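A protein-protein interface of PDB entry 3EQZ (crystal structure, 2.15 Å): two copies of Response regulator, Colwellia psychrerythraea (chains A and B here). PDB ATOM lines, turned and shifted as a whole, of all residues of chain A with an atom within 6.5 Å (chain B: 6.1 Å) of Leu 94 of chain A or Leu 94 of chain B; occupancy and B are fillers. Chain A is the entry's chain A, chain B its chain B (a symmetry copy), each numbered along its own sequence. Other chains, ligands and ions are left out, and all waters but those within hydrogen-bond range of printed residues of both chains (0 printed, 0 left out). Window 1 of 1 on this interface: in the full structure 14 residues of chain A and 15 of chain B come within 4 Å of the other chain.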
ATOM      1  N   MET A  56      30.975   8.477  17.264  1.00  0.00           N
ATOM      2  CA  MET A  56      31.858   8.796  16.134  1.00  0.00           C
ATOM      3  C   MET A  56      32.750  10.012  16.530  1.00  0.00           C
ATOM      4  O   MET A  56      32.310  10.890  17.290  1.00  0.00           O
ATOM      5  CB  MET A  56      31.034   9.108  14.869  1.00  0.00           C
ATOM      6  CG  MET A  56      30.149   7.926  14.296  1.00  0.00           C
ATOM      7  SD  MET A  56      31.139   6.595  13.521  1.00  0.00           S
ATOM      8  CE  MET A  56      31.775   7.472  12.112  1.00  0.00           C
ATOM      9  N   MET A  59      34.017   5.327  16.755  1.00  0.00           N
ATOM     10  CA  MET A  59      33.394   4.003  16.458  1.00  0.00           C
ATOM     11  C   MET A  59      33.282   2.932  17.589  1.00  0.00           C
ATOM     12  O   MET A  59      33.195   1.726  17.309  1.00  0.00           O
ATOM     13  CB  MET A  59      34.165   3.369  15.316  1.00  0.00           C
ATOM     14  CG  MET A  59      34.400   4.337  14.144  1.00  0.00           C
ATOM     15  SD  MET A  59      35.210   3.373  12.887  1.00  0.00           S
ATOM     16  CE  MET A  59      33.782   2.379  12.503  1.00  0.00           C
ATOM     17  N   ILE A  62      29.945   1.499  16.949  1.00  0.00           N
ATOM     18  CA  ILE A  62      29.942   0.463  15.883  1.00  0.00           C
ATOM     19  C   ILE A  62      30.341  -0.911  16.496  1.00  0.00           C
ATOM     20  O   ILE A  62      29.730  -1.939  16.196  1.00  0.00           O
ATOM     21  CB  ILE A  62      30.881   0.893  14.713  1.00  0.00           C
ATOM     22  CG1 ILE A  62      30.474   2.271  14.179  1.00  0.00           C
ATOM     23  CG2 ILE A  62      30.909  -0.151  13.591  1.00  0.00           C
ATOM     24  CD1 ILE A  62      29.079   2.321  13.604  1.00  0.00           C
ATOM     25  N   ILE A  65      27.351  -2.340  18.315  1.00  0.00           N
ATOM     26  CA  ILE A  65      26.394  -2.965  17.376  1.00  0.00           C
ATOM     27  C   ILE A  65      26.932  -4.339  16.858  1.00  0.00           C
ATOM     28  O   ILE A  65      26.171  -5.289  16.755  1.00  0.00           O
ATOM     29  CB  ILE A  65      26.059  -2.031  16.185  1.00  0.00           C
ATOM     30  CG1 ILE A  65      25.155  -0.849  16.638  1.00  0.00           C
ATOM     31  CG2 ILE A  65      25.409  -2.821  14.998  1.00  0.00           C
ATOM     32  CD1 ILE A  65      25.438   0.423  15.842  1.00  0.00           C
ATOM     33  N   GLY A  86      23.513  11.224   7.977  1.00  0.00           N
ATOM     34  CA  GLY A  86      23.565  10.196   6.938  1.00  0.00           C
ATOM     35  C   GLY A  86      24.236   8.956   7.555  1.00  0.00           C
ATOM     36  O   GLY A  86      23.870   7.853   7.295  1.00  0.00           O
ATOM     37  N   VAL A  87      25.261   9.180   8.369  1.00  0.00           N
ATOM     38  CA  VAL A  87      25.967   8.130   9.102  1.00  0.00           C
ATOM     39  C   VAL A  87      25.055   7.421  10.109  1.00  0.00           C
ATOM     40  O   VAL A  87      25.028   6.186  10.201  1.00  0.00           O
ATOM     41  CB  VAL A  87      27.246   8.736   9.788  1.00  0.00           C
ATOM     42  CG1 VAL A  87      27.876   7.729  10.769  1.00  0.00           C
ATOM     43  CG2 VAL A  87      28.282   9.154   8.702  1.00  0.00           C
ATOM     44  N   HIS A  89      21.742   7.228   9.953  1.00  0.00           N
ATOM     45  CA  HIS A  89      20.790   6.401   9.171  1.00  0.00           C
ATOM     46  C   HIS A  89      21.467   5.142   8.552  1.00  0.00           C
ATOM     47  O   HIS A  89      20.880   4.077   8.492  1.00  0.00           O
ATOM     48  CB  HIS A  89      20.118   7.254   8.068  1.00  0.00           C
ATOM     49  CG  HIS A  89      19.196   6.471   7.173  1.00  0.00           C
ATOM     50  ND1 HIS A  89      17.989   5.950   7.599  1.00  0.00           N
ATOM     51  CD2 HIS A  89      19.274   6.186   5.845  1.00  0.00           C
ATOM     52  CE1 HIS A  89      17.380   5.353   6.585  1.00  0.00           C
ATOM     53  NE2 HIS A  89      18.132   5.496   5.503  1.00  0.00           N
ATOM     54  N   SER A  90      22.702   5.284   8.078  1.00  0.00           N
ATOM     55  CA  SER A  90      23.459   4.073   7.657  1.00  0.00           C
ATOM     56  C   SER A  90      23.590   3.001   8.776  1.00  0.00           C
ATOM     57  O   SER A  90      23.317   1.815   8.554  1.00  0.00           O
ATOM     58  CB  SER A  90      24.817   4.497   7.147  1.00  0.00           C
ATOM     59  OG  SER A  90      24.605   5.464   6.134  1.00  0.00           O
ATOM     60  N   ALA A  91      23.943   3.430   9.995  1.00  0.00           N
ATOM     61  CA  ALA A  91      24.111   2.480  11.121  1.00  0.00           C
ATOM     62  C   ALA A  91      22.788   1.798  11.425  1.00  0.00           C
ATOM     63  O   ALA A  91      22.742   0.600  11.677  1.00  0.00           O
ATOM     64  CB  ALA A  91      24.675   3.201  12.358  1.00  0.00           C
ATOM     65  N   GLU A  92      21.692   2.526  11.331  1.00  0.00           N
ATOM     66  CA  GLU A  92      20.384   1.932  11.568  1.00  0.00           C
ATOM     67  C   GLU A  92      20.130   0.863  10.520  1.00  0.00           C
ATOM     68  O   GLU A  92      19.688  -0.233  10.840  1.00  0.00           O
ATOM     69  CB  GLU A  92      19.266   2.982  11.466  1.00  0.00           C
ATOM     70  CG  GLU A  92      17.858   2.352  11.572  1.00  0.00           C
ATOM     71  CD  GLU A  92      16.665   3.343  11.403  1.00  0.00           C
ATOM     72  OE1 GLU A  92      16.813   4.398  10.745  1.00  0.00           O
ATOM     73  OE2 GLU A  92      15.565   3.061  11.946  1.00  0.00           O
ATOM     74  N   THR A  93      20.396   1.214   9.250  1.00  0.00           N
ATOM     75  CA  THR A  93      20.180   0.290   8.123  1.00  0.00           C
ATOM     76  C   THR A  93      21.019  -0.976   8.302  1.00  0.00           C
ATOM     77  O   THR A  93      20.508  -2.099   8.196  1.00  0.00           O
ATOM     78  CB  THR A  93      20.470   0.986   6.724  1.00  0.00           C
ATOM     79  OG1 THR A  93      19.617   2.120   6.574  1.00  0.00           O
ATOM     80  CG2 THR A  93      20.211   0.023   5.519  1.00  0.00           C
ATOM     81  N   LEU A  94      22.296  -0.784   8.640  1.00  0.00           N
ATOM     82  CA  LEU A  94      23.203  -1.928   8.832  1.00  0.00           C
ATOM     83  C   LEU A  94      22.755  -2.798   9.989  1.00  0.00           C
ATOM     84  O   LEU A  94      22.745  -4.025   9.890  1.00  0.00           O
ATOM     85  CB  LEU A  94      24.625  -1.415   9.062  1.00  0.00           C
ATOM     86  CG  LEU A  94      25.239  -0.798   7.788  1.00  0.00           C
ATOM     87  CD1 LEU A  94      26.463  -0.097   8.147  1.00  0.00           C
ATOM     88  CD2 LEU A  94      25.532  -1.888   6.785  1.00  0.00           C
ATOM     89  N   ALA A  95      22.374  -2.163  11.103  1.00  0.00           N
ATOM     90  CA  ALA A  95      21.989  -2.920  12.298  1.00  0.00           C
ATOM     91  C   ALA A  95      20.686  -3.690  12.088  1.00  0.00           C
ATOM     92  O   ALA A  95      20.535  -4.801  12.553  1.00  0.00           O
ATOM     93  CB  ALA A  95      21.919  -1.989  13.543  1.00  0.00           C
ATOM     94  N   LEU A  96      19.744  -3.119  11.358  1.00  0.00           N
ATOM     95  CA  LEU A  96      18.508  -3.846  11.067  1.00  0.00           C
ATOM     96  C   LEU A  96      18.737  -5.061  10.147  1.00  0.00           C
ATOM     97  O   LEU A  96      18.110  -6.113  10.270  1.00  0.00           O
ATOM     98  CB  LEU A  96      17.539  -2.931  10.345  1.00  0.00           C
ATOM     99  CG  LEU A  96      16.764  -1.944  11.210  1.00  0.00           C
ATOM    100  CD1 LEU A  96      16.161  -0.843  10.299  1.00  0.00           C
ATOM    101  CD2 LEU A  96      15.674  -2.709  11.991  1.00  0.00           C
ATOM    102  N   SER A  97      19.642  -4.868   9.193  1.00  0.00           N
ATOM    103  CA  SER A  97      19.900  -5.873   8.186  1.00  0.00           C
ATOM    104  C   SER A  97      20.669  -7.033   8.819  1.00  0.00           C
ATOM    105  O   SER A  97      20.554  -8.159   8.373  1.00  0.00           O
ATOM    106  CB  SER A  97      20.646  -5.202   7.035  1.00  0.00           C
ATOM    107  OG  SER A  97      21.553  -6.100   6.478  1.00  0.00           O
ATOM    108  N   CYS A  98      21.427  -6.756   9.887  1.00  0.00           N
ATOM    109  CA  CYS A  98      22.052  -7.811  10.686  1.00  0.00           C
ATOM    110  C   CYS A  98      21.096  -8.405  11.701  1.00  0.00           C
ATOM    111  O   CYS A  98      21.531  -9.135  12.591  1.00  0.00           O
ATOM    112  CB  CYS A  98      23.271  -7.294  11.420  1.00  0.00           C
ATOM    113  SG  CYS A  98      24.617  -6.978  10.290  1.00  0.00           S
ATOM    114  N   GLY A  99      19.809  -8.058  11.592  1.00  0.00           N
ATOM    115  CA  GLY A  99      18.799  -8.649  12.440  1.00  0.00           C
ATOM    116  C   GLY A  99      18.551  -8.060  13.836  1.00  0.00           C
ATOM    117  O   GLY A  99      17.765  -8.640  14.616  1.00  0.00           O
ATOM    118  N   LEU A 100      19.193  -6.934  14.175  1.00  0.00           N
ATOM    119  CA  LEU A 100      18.915  -6.270  15.449  1.00  0.00           C
ATOM    120  C   LEU A 100      17.617  -5.495  15.385  1.00  0.00           C
ATOM    121  O   LEU A 100      17.265  -4.947  14.338  1.00  0.00           O
ATOM    122  CB  LEU A 100      20.024  -5.307  15.812  1.00  0.00           C
ATOM    123  CG  LEU A 100      21.387  -5.920  16.060  1.00  0.00           C
ATOM    124  CD1 LEU A 100      22.352  -4.801  16.303  1.00  0.00           C
ATOM    125  CD2 LEU A 100      21.301  -6.815  17.249  1.00  0.00           C
ATOM    126  N   LEU B  54      30.357  -7.848   2.337  1.00  0.00           N
ATOM    127  CA  LEU B  54      29.842  -7.404   3.620  1.00  0.00           C
ATOM    128  C   LEU B  54      29.392  -8.588   4.455  1.00  0.00           C
ATOM    129  O   LEU B  54      29.250  -8.477   5.652  1.00  0.00           O
ATOM    130  CB  LEU B  54      28.654  -6.453   3.456  1.00  0.00           C
ATOM    131  CG  LEU B  54      28.929  -5.068   2.878  1.00  0.00           C
ATOM    132  CD1 LEU B  54      27.618  -4.282   2.887  1.00  0.00           C
ATOM    133  CD2 LEU B  54      30.038  -4.319   3.606  1.00  0.00           C
ATOM    134  N   MET B  56      26.558 -10.029   4.773  1.00  0.00           N
ATOM    135  CA  MET B  56      25.266  -9.872   5.457  1.00  0.00           C
ATOM    136  C   MET B  56      24.643 -11.282   5.409  1.00  0.00           C
ATOM    137  O   MET B  56      24.794 -11.976   4.386  1.00  0.00           O
ATOM    138  CB  MET B  56      24.381  -8.859   4.722  1.00  0.00           C
ATOM    139  CG  MET B  56      24.751  -7.376   4.959  1.00  0.00           C
ATOM    140  SD  MET B  56      24.531  -6.906   6.675  1.00  0.00           S
ATOM    141  CE  MET B  56      26.128  -6.321   7.087  1.00  0.00           C
ATOM    142  N   MET B  59      27.864  -9.718  10.977  1.00  0.00           N
ATOM    143  CA  MET B  59      28.483  -8.368  11.020  1.00  0.00           C
ATOM    144  C   MET B  59      29.987  -8.440  10.750  1.00  0.00           C
ATOM    145  O   MET B  59      30.702  -7.466  10.967  1.00  0.00           O
ATOM    146  CB  MET B  59      28.182  -7.559  12.318  1.00  0.00           C
ATOM    147  CG  MET B  59      26.866  -6.717  12.387  1.00  0.00           C
ATOM    148  SD  MET B  59      26.710  -4.940  11.919  1.00  0.00           S
ATOM    149  CE  MET B  59      28.274  -4.250  12.444  1.00  0.00           C
ATOM    150  N   ILE B  62      31.213  -5.479   8.529  1.00  0.00           N
ATOM    151  CA  ILE B  62      31.314  -4.287   9.363  1.00  0.00           C
ATOM    152  C   ILE B  62      32.522  -4.289  10.282  1.00  0.00           C
ATOM    153  O   ILE B  62      33.164  -3.257  10.481  1.00  0.00           O
ATOM    154  CB  ILE B  62      30.030  -4.092  10.192  1.00  0.00           C
ATOM    155  CG1 ILE B  62      28.835  -4.161   9.243  1.00  0.00           C
ATOM    156  CG2 ILE B  62      30.042  -2.711  10.834  1.00  0.00           C
ATOM    157  CD1 ILE B  62      29.045  -3.318   7.976  1.00  0.00           C
ATOM    158  N   ILE B  65      35.625  -3.290   8.307  1.00  0.00           N
ATOM    159  CA  ILE B  65      35.598  -1.836   8.106  1.00  0.00           C
ATOM    160  C   ILE B  65      36.029  -1.082   9.345  1.00  0.00           C
ATOM    161  O   ILE B  65      36.910  -0.212   9.277  1.00  0.00           O
ATOM    162  CB  ILE B  65      34.184  -1.371   7.645  1.00  0.00           C
ATOM    163  CG1 ILE B  65      33.955  -1.825   6.205  1.00  0.00           C
ATOM    164  CG2 ILE B  65      34.034   0.151   7.784  1.00  0.00           C
ATOM    165  CD1 ILE B  65      32.500  -1.654   5.751  1.00  0.00           C
ATOM    166  N   VAL B  87      21.616  -1.149   1.959  1.00  0.00           N
ATOM    167  CA  VAL B  87      22.662  -1.777   2.790  1.00  0.00           C
ATOM    168  C   VAL B  87      24.076  -1.491   2.255  1.00  0.00           C
ATOM    169  O   VAL B  87      24.971  -1.107   2.993  1.00  0.00           O
ATOM    170  CB  VAL B  87      22.460  -3.298   3.009  1.00  0.00           C
ATOM    171  CG1 VAL B  87      23.601  -3.899   3.817  1.00  0.00           C
ATOM    172  CG2 VAL B  87      21.147  -3.602   3.725  1.00  0.00           C
ATOM    173  N   LEU B  88      24.262  -1.609   0.939  1.00  0.00           N
ATOM    174  CA  LEU B  88      25.569  -1.365   0.367  1.00  0.00           C
ATOM    175  C   LEU B  88      25.923   0.114   0.463  1.00  0.00           C
ATOM    176  O   LEU B  88      27.068   0.471   0.779  1.00  0.00           O
ATOM    177  CB  LEU B  88      25.555  -1.830  -1.084  1.00  0.00           C
ATOM    178  CG  LEU B  88      26.906  -1.913  -1.797  1.00  0.00           C
ATOM    179  CD1 LEU B  88      28.004  -2.744  -1.041  1.00  0.00           C
ATOM    180  CD2 LEU B  88      26.645  -2.465  -3.206  1.00  0.00           C
ATOM    181  N   HIS B  89      24.949   0.993   0.174  1.00  0.00           N
ATOM    182  CA  HIS B  89      25.171   2.422   0.303  1.00  0.00           C
ATOM    183  C   HIS B  89      25.478   2.834   1.760  1.00  0.00           C
ATOM    184  O   HIS B  89      26.277   3.718   2.006  1.00  0.00           O
ATOM    185  CB  HIS B  89      23.961   3.202  -0.260  1.00  0.00           C
ATOM    186  CG  HIS B  89      24.020   4.665   0.001  1.00  0.00           C
ATOM    187  ND1 HIS B  89      23.444   5.246   1.116  1.00  0.00           N
ATOM    188  CD2 HIS B  89      24.614   5.672  -0.687  1.00  0.00           C
ATOM    189  CE1 HIS B  89      23.677   6.550   1.105  1.00  0.00           C
ATOM    190  NE2 HIS B  89      24.393   6.832   0.023  1.00  0.00           N
ATOM    191  N   SER B  90      24.833   2.189   2.730  1.00  0.00           N
ATOM    192  CA  SER B  90      25.122   2.433   4.154  1.00  0.00           C
ATOM    193  C   SER B  90      26.581   2.122   4.555  1.00  0.00           C
ATOM    194  O   SER B  90      27.230   2.921   5.235  1.00  0.00           O
ATOM    195  CB  SER B  90      24.164   1.632   5.030  1.00  0.00           C
ATOM    196  OG  SER B  90      22.862   2.165   4.853  1.00  0.00           O
ATOM    197  N   ALA B  91      27.068   0.970   4.121  1.00  0.00           N
ATOM    198  CA  ALA B  91      28.445   0.530   4.378  1.00  0.00           C
ATOM    199  C   ALA B  91      29.399   1.473   3.705  1.00  0.00           C
ATOM    200  O   ALA B  91      30.442   1.865   4.285  1.00  0.00           O
ATOM    201  CB  ALA B  91      28.658  -0.895   3.816  1.00  0.00           C
ATOM    202  N   GLU B  92      29.089   1.851   2.463  1.00  0.00           N
ATOM    203  CA  GLU B  92      29.964   2.783   1.797  1.00  0.00           C
ATOM    204  C   GLU B  92      30.007   4.119   2.566  1.00  0.00           C
ATOM    205  O   GLU B  92      31.088   4.699   2.791  1.00  0.00           O
ATOM    206  CB  GLU B  92      29.473   3.022   0.363  1.00  0.00           C
ATOM    207  CG  GLU B  92      30.245   4.045  -0.408  1.00  0.00           C
ATOM    208  CD  GLU B  92      29.616   4.269  -1.816  1.00  0.00           C
ATOM    209  OE1 GLU B  92      28.430   3.910  -2.021  1.00  0.00           O
ATOM    210  OE2 GLU B  92      30.326   4.750  -2.710  1.00  0.00           O
ATOM    211  N   THR B  93      28.835   4.613   2.972  1.00  0.00           N
ATOM    212  CA  THR B  93      28.778   5.893   3.703  1.00  0.00           C
ATOM    213  C   THR B  93      29.533   5.807   5.020  1.00  0.00           C
ATOM    214  O   THR B  93      30.276   6.736   5.417  1.00  0.00           O
ATOM    215  CB  THR B  93      27.310   6.270   4.006  1.00  0.00           C
ATOM    216  OG1 THR B  93      26.596   6.382   2.759  1.00  0.00           O
ATOM    217  CG2 THR B  93      27.212   7.617   4.817  1.00  0.00           C
ATOM    218  N   LEU B  94      29.304   4.705   5.742  1.00  0.00           N
ATOM    219  CA  LEU B  94      30.037   4.506   7.008  1.00  0.00           C
ATOM    220  C   LEU B  94      31.534   4.512   6.743  1.00  0.00           C
ATOM    221  O   LEU B  94      32.279   5.218   7.397  1.00  0.00           O
ATOM    222  CB  LEU B  94      29.612   3.192   7.638  1.00  0.00           C
ATOM    223  CG  LEU B  94      30.189   2.802   9.001  1.00  0.00           C
ATOM    224  CD1 LEU B  94      29.962   3.891  10.117  1.00  0.00           C
ATOM    225  CD2 LEU B  94      29.668   1.443   9.476  1.00  0.00           C
ATOM    226  N   ALA B  95      31.983   3.733   5.756  1.00  0.00           N
ATOM    227  CA  ALA B  95      33.423   3.584   5.486  1.00  0.00           C
ATOM    228  C   ALA B  95      34.090   4.872   5.031  1.00  0.00           C
ATOM    229  O   ALA B  95      35.213   5.219   5.502  1.00  0.00           O
ATOM    230  CB  ALA B  95      33.687   2.459   4.434  1.00  0.00           C
ATOM    231  N   LEU B  96      33.443   5.582   4.103  1.00  0.00           N
ATOM    232  CA  LEU B  96      33.946   6.912   3.714  1.00  0.00           C
ATOM    233  C   LEU B  96      33.994   7.873   4.902  1.00  0.00           C
ATOM    234  O   LEU B  96      34.927   8.656   5.063  1.00  0.00           O
ATOM    235  CB  LEU B  96      33.035   7.526   2.660  1.00  0.00           C
ATOM    236  CG  LEU B  96      33.031   6.801   1.319  1.00  0.00           C
ATOM    237  CD1 LEU B  96      31.862   7.345   0.416  1.00  0.00           C
ATOM    238  CD2 LEU B  96      34.402   7.053   0.730  1.00  0.00           C
ATOM    239  N   SER B  97      32.963   7.842   5.724  1.00  0.00           N
ATOM    240  CA  SER B  97      32.990   8.695   6.886  1.00  0.00           C
ATOM    241  C   SER B  97      34.141   8.420   7.863  1.00  0.00           C
ATOM    242  O   SER B  97      34.603   9.329   8.567  1.00  0.00           O
ATOM    243  CB  SER B  97      31.708   8.532   7.652  1.00  0.00           C
ATOM    244  OG  SER B  97      31.791   9.467   8.685  1.00  0.00           O
ATOM    245  N   CYS B  98      34.578   7.168   7.940  1.00  0.00           N
ATOM    246  CA  CYS B  98      35.646   6.817   8.858  1.00  0.00           C
ATOM    247  C   CYS B  98      36.982   7.065   8.220  1.00  0.00           C
ATOM    248  O   CYS B  98      38.006   6.655   8.756  1.00  0.00           O
ATOM    249  CB  CYS B  98      35.568   5.356   9.236  1.00  0.00           C
ATOM    250  SG  CYS B  98      34.097   4.972  10.094  1.00  0.00           S
ATOM    251  N   GLY B  99      36.981   7.694   7.051  1.00  0.00           N
ATOM    252  CA  GLY B  99      38.234   8.040   6.411  1.00  0.00           C
ATOM    253  C   GLY B  99      38.813   6.973   5.504  1.00  0.00           C
ATOM    254  O   GLY B  99      39.978   7.082   5.099  1.00  0.00           O
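Printed residues of chain B within 4 Å of Leu 94 of chain A: Ile 62 (3.98 Å), Val 87 (3.9 Å), Ser 90 (3.8 Å) and Leu 94 (3.8 Å).
Leu 94 of chain B touches just these residues of chain A: Ile 62 and Leu 94.
Printed residues of chain A within 4 Å of Cys 98 of chain B: Met 56 and Met 59.
Of the printed residues of chain A, Ile 62 of chain B touches Ile 62 (3.9 Å) and Leu 94 (3.98 Å).
Printed residues of chain A within 4 Å of Met 59 of chain B: Ile 65 and Cys 98.
Of the printed residues of chain B, Ile 65 of chain A touches Met 59 (3.96 Å).
Ile 65 of chain B touches none of the printed residues of chain A.
Leu 88 of chain B touches none of the printed residues of chain A.
The nearest printed residue of chain B that does not touch Thr 93 of chain A is Val 87 of chain B (4.003 Å).
Ser 97 of chain B touches Met 56 of chain A.
SG of Cys 98 of chain B touches CE of Met 56 of chain A, 3.96 Å away.
Leu 94 of chain B touches Ile 62 of chain A (CD1 to CD1, 3.9 Å).
Ser 97 of chain B touches Val 87 of chain A.
OG of Ser 90 of chain A touches CB of Thr 93 of chain B, 3.5 Å away.
CB of Thr 93 of chain A touches OG of Ser 90 of chain B (3.3 Å).
CD2 of Leu 94 of chain A touches CD1 of Ile 62 of chain B (3.98 Å).
CD2 of Leu 94 of chain A touches O of Val 87 of chain B, 3.9 Å away.
Leu 94 of chain A touches Ser 90 of chain B.
Val 87 of chain B touches Ser 97 of chain A (CG2 to CB, 3.7 Å).
The side-chain sulfur (SD) of Met 59 of chain A is in hydrogen-bond range of the side-chain sulfur (SG) of Cys 98 of chain B (3.4 Å).
OG of Ser 97 of chain A lies within hydrogen-bond range of SD of Met 56 of chain B.
The side-chain sulfur (SD) of Met 56 of chain B sits close to the side-chain sulfur (SG) of Cys 98 of chain A (3.6 Å).
The side-chain sulfur of Cys 98 of chain A sits close to the side-chain sulfur of Met 59 of chain B, at 3.3 Å.
Among the printed residues, 18 pairs touch across the chains.
Met 56 of chain A touches Ser 97 of chain B, and with the chains exchanged Ser 97 of chain A touches Met 56 of chain B.
Met 59 of chain A touches Cys 98 of chain B, and with the chains exchanged Cys 98 of chain A touches Met 59 of chain B.
Ser 90 of chain B touches its own counterpart, Ser 90 of chain A.
Leu 94 of chain A touches Val 87 of chain B, but with the chains exchanged Val 87 of chain A does not touch Leu 94 of chain B (4.4 Å).
The backbone carbonyl oxygen (O) of Gly 86 of chain A sits at hydrogen-bond distance from the side-chain hydroxyl (OG) of Ser 90 of chain A, at 2.8 Å.
The side-chain hydroxyl (OG1) of Thr 93 of chain A is in hydrogen-bond range of the backbone carbonyl oxygen (O) of His 89 of chain A, at 3.0 Å.
O of Leu 94 of chain A is in hydrogen-bond range of SG of Cys 98 of chain A, 3.5 Å away.
O of His 89 of chain B sits at hydrogen-bond distance from OG1 of Thr 93 of chain B (2.8 Å).
The side-chain sulfur of Cys 98 of chain B is in hydrogen-bond range of the backbone carbonyl oxygen of Leu 94 of chain B (3.3 Å).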
